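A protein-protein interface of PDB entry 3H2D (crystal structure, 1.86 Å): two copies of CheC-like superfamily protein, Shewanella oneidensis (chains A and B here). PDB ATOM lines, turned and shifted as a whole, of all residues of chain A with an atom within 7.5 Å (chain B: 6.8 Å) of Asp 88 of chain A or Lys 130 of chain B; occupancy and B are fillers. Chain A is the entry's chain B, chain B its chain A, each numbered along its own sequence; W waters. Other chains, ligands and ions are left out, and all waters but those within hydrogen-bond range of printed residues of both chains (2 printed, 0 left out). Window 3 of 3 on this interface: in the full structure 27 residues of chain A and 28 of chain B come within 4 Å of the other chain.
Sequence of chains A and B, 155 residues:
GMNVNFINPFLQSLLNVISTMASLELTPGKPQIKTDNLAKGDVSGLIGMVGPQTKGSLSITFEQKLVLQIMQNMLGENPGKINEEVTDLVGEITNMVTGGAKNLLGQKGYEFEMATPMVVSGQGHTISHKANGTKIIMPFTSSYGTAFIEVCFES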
ATOM      1  N   VAL A  43     -13.044  -6.172  18.824  1.00  0.00           N
ATOM      2  CA  VAL A  43     -12.078  -5.672  19.826  1.00  0.00           C
ATOM      3  C   VAL A  43     -11.172  -4.677  19.121  1.00  0.00           C
ATOM      4  O   VAL A  43     -10.771  -4.926  17.976  1.00  0.00           O
ATOM      5  CB  VAL A  43     -11.294  -6.838  20.496  1.00  0.00           C
ATOM      6  CG1 VAL A  43     -10.355  -7.602  19.515  1.00  0.00           C
ATOM      7  CG2 VAL A  43     -10.530  -6.300  21.723  1.00  0.00           C
ATOM      8  N   LEU A  75       0.560 -16.732  21.508  1.00  0.00           N
ATOM      9  CA  LEU A  75       0.650 -17.227  22.906  1.00  0.00           C
ATOM     10  C   LEU A  75       0.313 -18.715  23.108  1.00  0.00           C
ATOM     11  O   LEU A  75       0.516 -19.251  24.176  1.00  0.00           O
ATOM     12  CB  LEU A  75      -0.244 -16.368  23.821  1.00  0.00           C
ATOM     13  CG  LEU A  75       0.011 -14.857  23.795  1.00  0.00           C
ATOM     14  CD1 LEU A  75      -1.077 -14.127  24.593  1.00  0.00           C
ATOM     15  CD2 LEU A  75       1.457 -14.521  24.291  1.00  0.00           C
ATOM     16  N   ASN A  83     -11.753 -11.873  26.345  1.00  0.00           N
ATOM     17  CA  ASN A  83     -11.684 -11.662  27.799  1.00  0.00           C
ATOM     18  C   ASN A  83     -10.491 -10.736  28.095  1.00  0.00           C
ATOM     19  O   ASN A  83      -9.930 -10.158  27.145  1.00  0.00           O
ATOM     20  CB  ASN A  83     -11.602 -12.986  28.547  1.00  0.00           C
ATOM     21  CG  ASN A  83     -10.377 -13.802  28.203  1.00  0.00           C
ATOM     22  OD1 ASN A  83      -9.439 -13.347  27.525  1.00  0.00           O
ATOM     23  ND2 ASN A  83     -10.388 -15.051  28.658  1.00  0.00           N
ATOM     24  N   GLU A  84     -10.134 -10.600  29.385  1.00  0.00           N
ATOM     25  CA  GLU A  84      -9.032  -9.737  29.798  1.00  0.00           C
ATOM     26  C   GLU A  84      -7.717 -10.176  29.189  1.00  0.00           C
ATOM     27  O   GLU A  84      -6.926  -9.330  28.835  1.00  0.00           O
ATOM     28  CB  GLU A  84      -8.888  -9.646  31.320  1.00  0.00           C
ATOM     29  CG  GLU A  84      -8.094  -8.406  31.835  1.00  0.00           C
ATOM     30  CD  GLU A  84      -7.886  -8.410  33.372  1.00  0.00           C
ATOM     31  N   GLU A  85      -7.451 -11.471  29.060  1.00  0.00           N
ATOM     32  CA  GLU A  85      -6.188 -11.868  28.427  1.00  0.00           C
ATOM     33  C   GLU A  85      -6.128 -11.424  26.976  1.00  0.00           C
ATOM     34  O   GLU A  85      -5.053 -11.071  26.485  1.00  0.00           O
ATOM     35  CB  GLU A  85      -5.966 -13.374  28.536  1.00  0.00           C
ATOM     36  CG  GLU A  85      -5.683 -13.832  29.985  1.00  0.00           C
ATOM     37  N   VAL A  86      -7.266 -11.460  26.292  1.00  0.00           N
ATOM     38  CA  VAL A  86      -7.327 -11.002  24.876  1.00  0.00           C
ATOM     39  C   VAL A  86      -7.109  -9.501  24.807  1.00  0.00           C
ATOM     40  O   VAL A  86      -6.306  -9.030  24.018  1.00  0.00           O
ATOM     41  CB  VAL A  86      -8.604 -11.426  24.128  1.00  0.00           C
ATOM     42  CG1 VAL A  86      -8.656 -10.815  22.664  1.00  0.00           C
ATOM     43  CG2 VAL A  86      -8.737 -12.953  24.074  1.00  0.00           C
ATOM     44  N   THR A  87      -7.785  -8.743  25.662  1.00  0.00           N
ATOM     45  CA  THR A  87      -7.613  -7.292  25.660  1.00  0.00           C
ATOM     46  C   THR A  87      -6.171  -6.878  26.042  1.00  0.00           C
ATOM     47  O   THR A  87      -5.642  -5.950  25.456  1.00  0.00           O
ATOM     48  CB  THR A  87      -8.674  -6.552  26.488  1.00  0.00           C
ATOM     49  OG1 THR A  87      -8.437  -6.742  27.900  1.00  0.00           O
ATOM     50  CG2 THR A  87     -10.126  -6.971  26.031  1.00  0.00           C
ATOM     51  N   ASP A  88      -5.550  -7.579  26.987  1.00  0.00           N
ATOM     52  CA  ASP A  88      -4.136  -7.353  27.280  1.00  0.00           C
ATOM     53  C   ASP A  88      -3.258  -7.539  26.025  1.00  0.00           C
ATOM     54  O   ASP A  88      -2.427  -6.703  25.734  1.00  0.00           O
ATOM     55  CB  ASP A  88      -3.649  -8.330  28.348  1.00  0.00           C
ATOM     56  CG  ASP A  88      -4.137  -7.997  29.718  1.00  0.00           C
ATOM     57  OD1 ASP A  88      -4.704  -6.910  29.969  1.00  0.00           O
ATOM     58  OD2 ASP A  88      -3.899  -8.846  30.576  1.00  0.00           O
ATOM     59  N   LEU A  89      -3.482  -8.597  25.256  1.00  0.00           N
ATOM     60  CA  LEU A  89      -2.680  -8.808  24.053  1.00  0.00           C
ATOM     61  C   LEU A  89      -2.909  -7.696  23.022  1.00  0.00           C
ATOM     62  O   LEU A  89      -1.969  -7.235  22.407  1.00  0.00           O
ATOM     63  CB  LEU A  89      -2.983 -10.169  23.402  1.00  0.00           C
ATOM     64  CG  LEU A  89      -2.149 -10.494  22.131  1.00  0.00           C
ATOM     65  CD1 LEU A  89      -0.646 -10.564  22.440  1.00  0.00           C
ATOM     66  CD2 LEU A  89      -2.607 -11.814  21.549  1.00  0.00           C
ATOM     67  N   VAL A  90      -4.154  -7.299  22.829  1.00  0.00           N
ATOM     68  CA  VAL A  90      -4.453  -6.211  21.910  1.00  0.00           C
ATOM     69  C   VAL A  90      -3.749  -4.923  22.357  1.00  0.00           C
ATOM     70  O   VAL A  90      -3.242  -4.155  21.517  1.00  0.00           O
ATOM     71  CB  VAL A  90      -5.978  -6.037  21.738  1.00  0.00           C
ATOM     72  CG1 VAL A  90      -6.315  -4.729  20.970  1.00  0.00           C
ATOM     73  CG2 VAL A  90      -6.558  -7.304  21.032  1.00  0.00           C
ATOM     74  N   GLY A  91      -3.703  -4.675  23.659  1.00  0.00           N
ATOM     75  CA  GLY A  91      -2.973  -3.535  24.209  1.00  0.00           C
ATOM     76  C   GLY A  91      -1.513  -3.600  23.852  1.00  0.00           C
ATOM     77  O   GLY A  91      -0.935  -2.599  23.430  1.00  0.00           O
ATOM     78  N   GLU A  92      -0.911  -4.775  23.988  1.00  0.00           N
ATOM     79  CA  GLU A  92       0.513  -4.949  23.650  1.00  0.00           C
ATOM     80  C   GLU A  92       0.765  -4.832  22.164  1.00  0.00           C
ATOM     81  O   GLU A  92       1.731  -4.209  21.763  1.00  0.00           O
ATOM     82  CB  GLU A  92       1.079  -6.276  24.176  1.00  0.00           C
ATOM     83  CG  GLU A  92       1.251  -6.304  25.687  1.00  0.00           C
ATOM     84  CD  GLU A  92       2.159  -5.141  26.174  1.00  0.00           C
ATOM     85  OE1 GLU A  92       3.170  -4.841  25.497  1.00  0.00           O
ATOM     86  OE2 GLU A  92       1.835  -4.491  27.194  1.00  0.00           O
ATOM     87  N   ILE A  93      -0.121  -5.370  21.348  1.00  0.00           N
ATOM     88  CA  ILE A  93      -0.016  -5.174  19.897  1.00  0.00           C
ATOM     89  C   ILE A  93      -0.092  -3.698  19.570  1.00  0.00           C
ATOM     90  O   ILE A  93       0.696  -3.173  18.748  1.00  0.00           O
ATOM     91  CB  ILE A  93      -1.131  -5.956  19.105  1.00  0.00           C
ATOM     92  CG1 ILE A  93      -0.888  -7.463  19.245  1.00  0.00           C
ATOM     93  CG2 ILE A  93      -1.166  -5.519  17.640  1.00  0.00           C
ATOM     94  CD1 ILE A  93      -2.003  -8.316  18.651  1.00  0.00           C
ATOM     95  N   THR A  94      -1.030  -2.996  20.212  1.00  0.00           N
ATOM     96  CA  THR A  94      -1.170  -1.554  19.983  1.00  0.00           C
ATOM     97  C   THR A  94       0.124  -0.790  20.319  1.00  0.00           C
ATOM     98  O   THR A  94       0.571   0.111  19.541  1.00  0.00           O
ATOM     99  CB  THR A  94      -2.348  -0.981  20.797  1.00  0.00           C
ATOM    100  OG1 THR A  94      -3.543  -1.648  20.412  1.00  0.00           O
ATOM    101  CG2 THR A  94      -2.519   0.498  20.547  1.00  0.00           C
ATOM    102  N   ASN A  95       0.722  -1.127  21.467  1.00  0.00           N
ATOM    103  CA  ASN A  95       1.975  -0.489  21.848  1.00  0.00           C
ATOM    104  C   ASN A  95       3.091  -0.781  20.838  1.00  0.00           C
ATOM    105  O   ASN A  95       3.884   0.114  20.524  1.00  0.00           O
ATOM    106  CB  ASN A  95       2.466  -0.964  23.209  1.00  0.00           C
ATOM    107  CG  ASN A  95       1.935  -0.169  24.340  1.00  0.00           C
ATOM    108  OD1 ASN A  95       1.650   1.026  24.213  1.00  0.00           O
ATOM    109  ND2 ASN A  95       1.799  -0.853  25.517  1.00  0.00           N
ATOM    110  N   THR A 116      -1.160   5.860  26.326  1.00  0.00           N
ATOM    111  CA  THR A 116      -1.254   4.484  26.736  1.00  0.00           C
ATOM    112  C   THR A 116      -2.504   3.818  26.091  1.00  0.00           C
ATOM    113  O   THR A 116      -3.490   4.474  25.840  1.00  0.00           O
ATOM    114  CB  THR A 116      -1.308   4.365  28.237  1.00  0.00           C
ATOM    115  OG1 THR A 116      -2.401   5.137  28.730  1.00  0.00           O
ATOM    116  CG2 THR A 116      -0.015   4.836  28.875  1.00  0.00           C
ATOM    117  N   PRO A 117      -2.444   2.497  25.849  1.00  0.00           N
ATOM    118  CA  PRO A 117      -3.525   1.897  25.102  1.00  0.00           C
ATOM    119  C   PRO A 117      -4.830   1.802  25.880  1.00  0.00           C
ATOM    120  O   PRO A 117      -4.831   1.641  27.081  1.00  0.00           O
ATOM    121  CB  PRO A 117      -3.040   0.471  24.841  1.00  0.00           C
ATOM    122  CG  PRO A 117      -1.584   0.523  25.019  1.00  0.00           C
ATOM    123  CD  PRO A 117      -1.400   1.501  26.143  1.00  0.00           C
ATOM    124  N   MET A 118      -5.928   2.001  25.170  1.00  0.00           N
ATOM    125  CA  MET A 118      -7.235   1.643  25.679  1.00  0.00           C
ATOM    126  C   MET A 118      -7.777   0.644  24.708  1.00  0.00           C
ATOM    127  O   MET A 118      -7.624   0.799  23.497  1.00  0.00           O
ATOM    128  CB  MET A 118      -8.157   2.843  25.739  1.00  0.00           C
ATOM    129  CG  MET A 118      -7.892   3.725  26.911  1.00  0.00           C
ATOM    130  SD  MET A 118      -8.820   5.397  26.681  1.00  0.00           S
ATOM    131  CE  MET A 118      -7.566   6.306  25.511  1.00  0.00           C
ATOM    132  N   VAL A 119      -8.367  -0.409  25.255  1.00  0.00           N
ATOM    133  CA  VAL A 119      -8.946  -1.477  24.450  1.00  0.00           C
ATOM    134  C   VAL A 119     -10.461  -1.552  24.630  1.00  0.00           C
ATOM    135  O   VAL A 119     -10.962  -1.648  25.749  1.00  0.00           O
ATOM    136  CB  VAL A 119      -8.293  -2.863  24.769  1.00  0.00           C
ATOM    137  CG1 VAL A 119      -8.829  -3.973  23.843  1.00  0.00           C
ATOM    138  CG2 VAL A 119      -6.759  -2.694  24.646  1.00  0.00           C
ATOM    139  N   VAL A 120     -11.152  -1.519  23.492  1.00  0.00           N
ATOM    140  CA  VAL A 120     -12.583  -1.559  23.401  1.00  0.00           C
ATOM    141  C   VAL A 120     -12.974  -2.988  23.107  1.00  0.00           C
ATOM    142  O   VAL A 120     -12.378  -3.618  22.239  1.00  0.00           O
ATOM    143  CB  VAL A 120     -13.050  -0.691  22.234  1.00  0.00           C
ATOM    144  CG1 VAL A 120     -14.586  -0.798  22.051  1.00  0.00           C
ATOM    145  CG2 VAL A 120     -12.542   0.783  22.419  1.00  0.00           C
ATOM    146  N   SER B  57      -4.577   8.007  30.003  1.00  0.00           N
ATOM    147  CA  SER B  57      -5.768   7.862  29.204  1.00  0.00           C
ATOM    148  C   SER B  57      -7.048   8.168  29.971  1.00  0.00           C
ATOM    149  O   SER B  57      -7.123   8.014  31.203  1.00  0.00           O
ATOM    150  CB  SER B  57      -5.828   6.438  28.673  1.00  0.00           C
ATOM    151  OG  SER B  57      -5.792   5.490  29.717  1.00  0.00           O
ATOM    152  N   SER B 128     -11.146  -1.049  28.451  1.00  0.00           N
ATOM    153  CA  SER B 128     -10.107  -1.509  29.368  1.00  0.00           C
ATOM    154  C   SER B 128      -8.839  -0.655  29.159  1.00  0.00           C
ATOM    155  O   SER B 128      -8.212  -0.708  28.083  1.00  0.00           O
ATOM    156  CB  SER B 128      -9.839  -2.996  29.106  1.00  0.00           C
ATOM    157  OG  SER B 128      -8.778  -3.481  29.933  1.00  0.00           O
ATOM    158  N   HIS B 129      -8.461   0.127  30.175  1.00  0.00           N
ATOM    159  CA  HIS B 129      -7.253   0.947  30.115  1.00  0.00           C
ATOM    160  C   HIS B 129      -6.051   0.111  30.514  1.00  0.00           C
ATOM    161  O   HIS B 129      -6.045  -0.566  31.550  1.00  0.00           O
ATOM    162  CB  HIS B 129      -7.348   2.177  31.031  1.00  0.00           C
ATOM    163  CG  HIS B 129      -8.406   3.142  30.650  1.00  0.00           C
ATOM    164  ND1 HIS B 129      -8.117   4.443  30.321  1.00  0.00           N
ATOM    165  CD2 HIS B 129      -9.741   2.999  30.499  1.00  0.00           C
ATOM    166  CE1 HIS B 129      -9.238   5.073  30.020  1.00  0.00           C
ATOM    167  NE2 HIS B 129     -10.238   4.222  30.112  1.00  0.00           N
ATOM    168  N   LYS B 130      -5.018   0.153  29.695  1.00  0.00           N
ATOM    169  CA  LYS B 130      -3.851  -0.713  29.869  1.00  0.00           C
ATOM    170  C   LYS B 130      -2.590  -0.018  30.441  1.00  0.00           C
ATOM    171  O   LYS B 130      -1.574  -0.680  30.712  1.00  0.00           O
ATOM    172  CB  LYS B 130      -3.528  -1.400  28.521  1.00  0.00           C
ATOM    173  CG  LYS B 130      -4.689  -2.182  27.939  1.00  0.00           C
ATOM    174  CD  LYS B 130      -5.055  -3.356  28.857  1.00  0.00           C
ATOM    175  CE  LYS B 130      -6.310  -4.035  28.403  1.00  0.00           C
ATOM    176  NZ  LYS B 130      -6.581  -5.288  29.203  1.00  0.00           N
ATOM    177  N   ALA B 131      -2.641   1.279  30.664  1.00  0.00           N
ATOM    178  CA  ALA B 131      -1.576   1.955  31.382  1.00  0.00           C
ATOM    179  C   ALA B 131      -1.163   1.196  32.634  1.00  0.00           C
ATOM    180  O   ALA B 131      -2.003   0.641  33.351  1.00  0.00           O
ATOM    181  CB  ALA B 131      -1.988   3.404  31.743  1.00  0.00           C
ATOM    182  N   ASN B 132       0.143   1.182  32.889  1.00  0.00           N
ATOM    183  CA  ASN B 132       0.708   0.599  34.095  1.00  0.00           C
ATOM    184  C   ASN B 132       0.593   1.595  35.239  1.00  0.00           C
ATOM    185  O   ASN B 132       1.559   2.258  35.608  1.00  0.00           O
ATOM    186  CB  ASN B 132       2.179   0.208  33.889  1.00  0.00           C
ATOM    187  CG  ASN B 132       2.751  -0.552  35.073  1.00  0.00           C
ATOM    188  N   GLY B 133      -0.609   1.717  35.768  1.00  0.00           N
ATOM    189  CA  GLY B 133      -0.875   2.544  36.945  1.00  0.00           C
ATOM    190  C   GLY B 133      -2.314   2.341  37.376  1.00  0.00           C
ATOM    191  O   GLY B 133      -3.048   1.506  36.812  1.00  0.00           O
ATOM    192  N   LYS B 135      -6.150   2.560  37.908  1.00  0.00           N
ATOM    193  CA  LYS B 135      -7.328   2.878  37.139  1.00  0.00           C
ATOM    194  C   LYS B 135      -8.415   3.382  38.076  1.00  0.00           C
ATOM    195  O   LYS B 135      -8.871   2.618  38.938  1.00  0.00           O
ATOM    196  CB  LYS B 135      -7.845   1.605  36.477  1.00  0.00           C
ATOM    197  CG  LYS B 135      -7.063   1.128  35.236  1.00  0.00           C
ATOM    198  CD  LYS B 135      -6.052   0.094  35.587  1.00  0.00           C
ATOM    199  CE  LYS B 135      -5.173  -0.236  34.385  1.00  0.00           C
ATOM    200  NZ  LYS B 135      -3.879  -0.822  34.780  1.00  0.00           N
ATOM    201  N   CYS B 152      -6.603   6.927  33.898  1.00  0.00           N
ATOM    202  CA  CYS B 152      -5.479   6.078  34.284  1.00  0.00           C
ATOM    203  C   CYS B 152      -4.186   6.773  33.876  1.00  0.00           C
ATOM    204  O   CYS B 152      -4.048   7.192  32.745  1.00  0.00           O
ATOM    205  CB  CYS B 152      -5.565   4.688  33.626  1.00  0.00           C
ATOM    206  SG  CYS B 152      -4.317   3.474  34.289  1.00  0.00           S
ATOM    207  N   GLU B 154       0.214   6.468  34.157  1.00  0.00           N
ATOM    208  CA  GLU B 154       1.335   5.558  34.348  1.00  0.00           C
ATOM    209  C   GLU B 154       2.526   6.418  34.659  1.00  0.00           C
ATOM    210  O   GLU B 154       2.730   7.397  33.918  1.00  0.00           O
ATOM    211  CB  GLU B 154       1.500   4.845  33.022  1.00  0.00           C
ATOM    212  CG  GLU B 154       2.788   4.319  32.694  1.00  0.00           C
ATOM    213  CD  GLU B 154       2.738   3.574  31.356  1.00  0.00           C
ATOM    214  OE1 GLU B 154       3.446   4.062  30.439  1.00  0.00           O
ATOM    215  OE2 GLU B 154       1.994   2.541  31.232  1.00  0.00           O
HETATM  216  O   HOH W   1       0.652  -0.455  28.453  1.00  0.00           O
HETATM  217  O   HOH W   2      -4.446   3.297  29.240  1.00  0.00           O
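Of the printed residues of chain B, Thr 87 of chain A touches Ser 128 and Lys 130.
Asp 88 of chain A touches just one residue of chain B: Lys 130.
Of the printed residues of chain B, Thr 116 of chain A touches Ser 57 (3.5 Å), Ala 131 (3.5 Å) and Glu 154 (3.9 Å).
Of the printed residues of chain B, Met 118 of chain A touches Ser 57, Ser 128 and His 129.
Printed residues of chain A within 4 Å of His 129 of chain B: Pro 117 and Met 118.
Lys 130 of chain B touches just these residues of chain A: Thr 87, Asp 88, Pro 117 and Val 119.
The nearest residue of chain A that does not touch Lys 130 of chain B is Glu 84 of chain A (4.1 Å).
No position is printed for both chains.
Of the 13 pairs that touch across the chains among the printed residues, none has its exchanged pair printed and touching as well.
Printed residues of chain B that touch a printed residue of chain A: Ser 57, Ser 128, His 129, Lys 130, Ala 131 and Glu 154.
Of the 20 printed residues of chain A, 6 touch a printed residue of chain B.
Printed residues of chain A that touch a printed residue of chain B: Thr 87, Asp 88, Thr 116, Pro 117, Met 118 and Val 119.
Hydrophobic or aromatic side chains of chain A within 4 Å of the printed part of chain B: Met 118 and Val 119.
Among the printed residues, Asp or Glu carboxylates within 4 Å of a Lys or Arg side-chain nitrogen of the other chain: Asp 88 of chain A with Lys 130 of chain B (2.6 Å).
Water W2 lies within hydrogen-bond range of the side-chain hydroxyl (OG) of Ser 57 of chain B, the backbone carbonyl oxygen (O) of Pro 117 of chain A, the side-chain hydroxyl (OG1) of Thr 116 of chain A, the backbone NH (N) of Ala 131 of chain B and the backbone NH (N) of Lys 130 of chain B.
Water W1 bridges ND2 of Asn 95 of chain A (3.2 Å) and O of Lys 130 of chain B (3.2 Å).
The side-chain hydroxyl (OG) of Ser 57 of chain B sits at hydrogen-bond distance from a ring nitrogen (ND1) of His 129 of chain B (2.6 Å).
N of Ser 57 of chain B is in hydrogen-bond range of O of Cys 152 of chain B (2.9 Å).
The backbone carbonyl oxygen of Ala 131 of chain B lies within hydrogen-bond range of the side-chain amino group of Lys 135 of chain B (2.8 Å).
The side-chain sulfur (SG) of Cys 152 of chain B lies close to the backbone carbonyl oxygen (O) of Ala 131 of chain B.
N of Asn 132 of chain B sits at hydrogen-bond distance from OE2 of Glu 154 of chain B (2.8 Å).
O of Glu 84 of chain A is in hydrogen-bond range of OG1 of Thr 87 of chain A (3.1 Å).
Thr 87 of chain A touches Ser 128 of chain B.
OG of Ser 57 of chain B touches OG1 of Thr 116 of chain A, 3.5 Å away.
Thr 116 of chain A touches Ala 131 of chain B.
Thr 116 of chain A touches Glu 154 of chain B.
CA of His 129 of chain B touches O of Pro 117 of chain A (3.9 Å).
Ser 57 of chain B touches Met 118 of chain A.
O of Ser 128 of chain B touches CA of Met 118 of chain A (3.5 Å).
Met 118 of chain A touches His 129 of chain B (SD to CE1, 3.4 Å).
CG of Lys 130 of chain B touches CG2 of Val 119 of chain A, 3.9 Å away.
N of Ser 128 of chain B sits at hydrogen-bond distance from O of Val 119 of chain A (2.8 Å).
OG1 of Thr 87 of chain A lies within hydrogen-bond range of NZ of Lys 130 of chain B (2.7 Å).
The side-chain amino group (NZ) of Lys 130 of chain B is in salt-bridge range of the side-chain carboxylate (OD1) of Asp 88 of chain A, at 2.6 Å.
O of Pro 117 of chain A lies within hydrogen-bond range of N of Lys 130 of chain B, 3.0 Å away.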
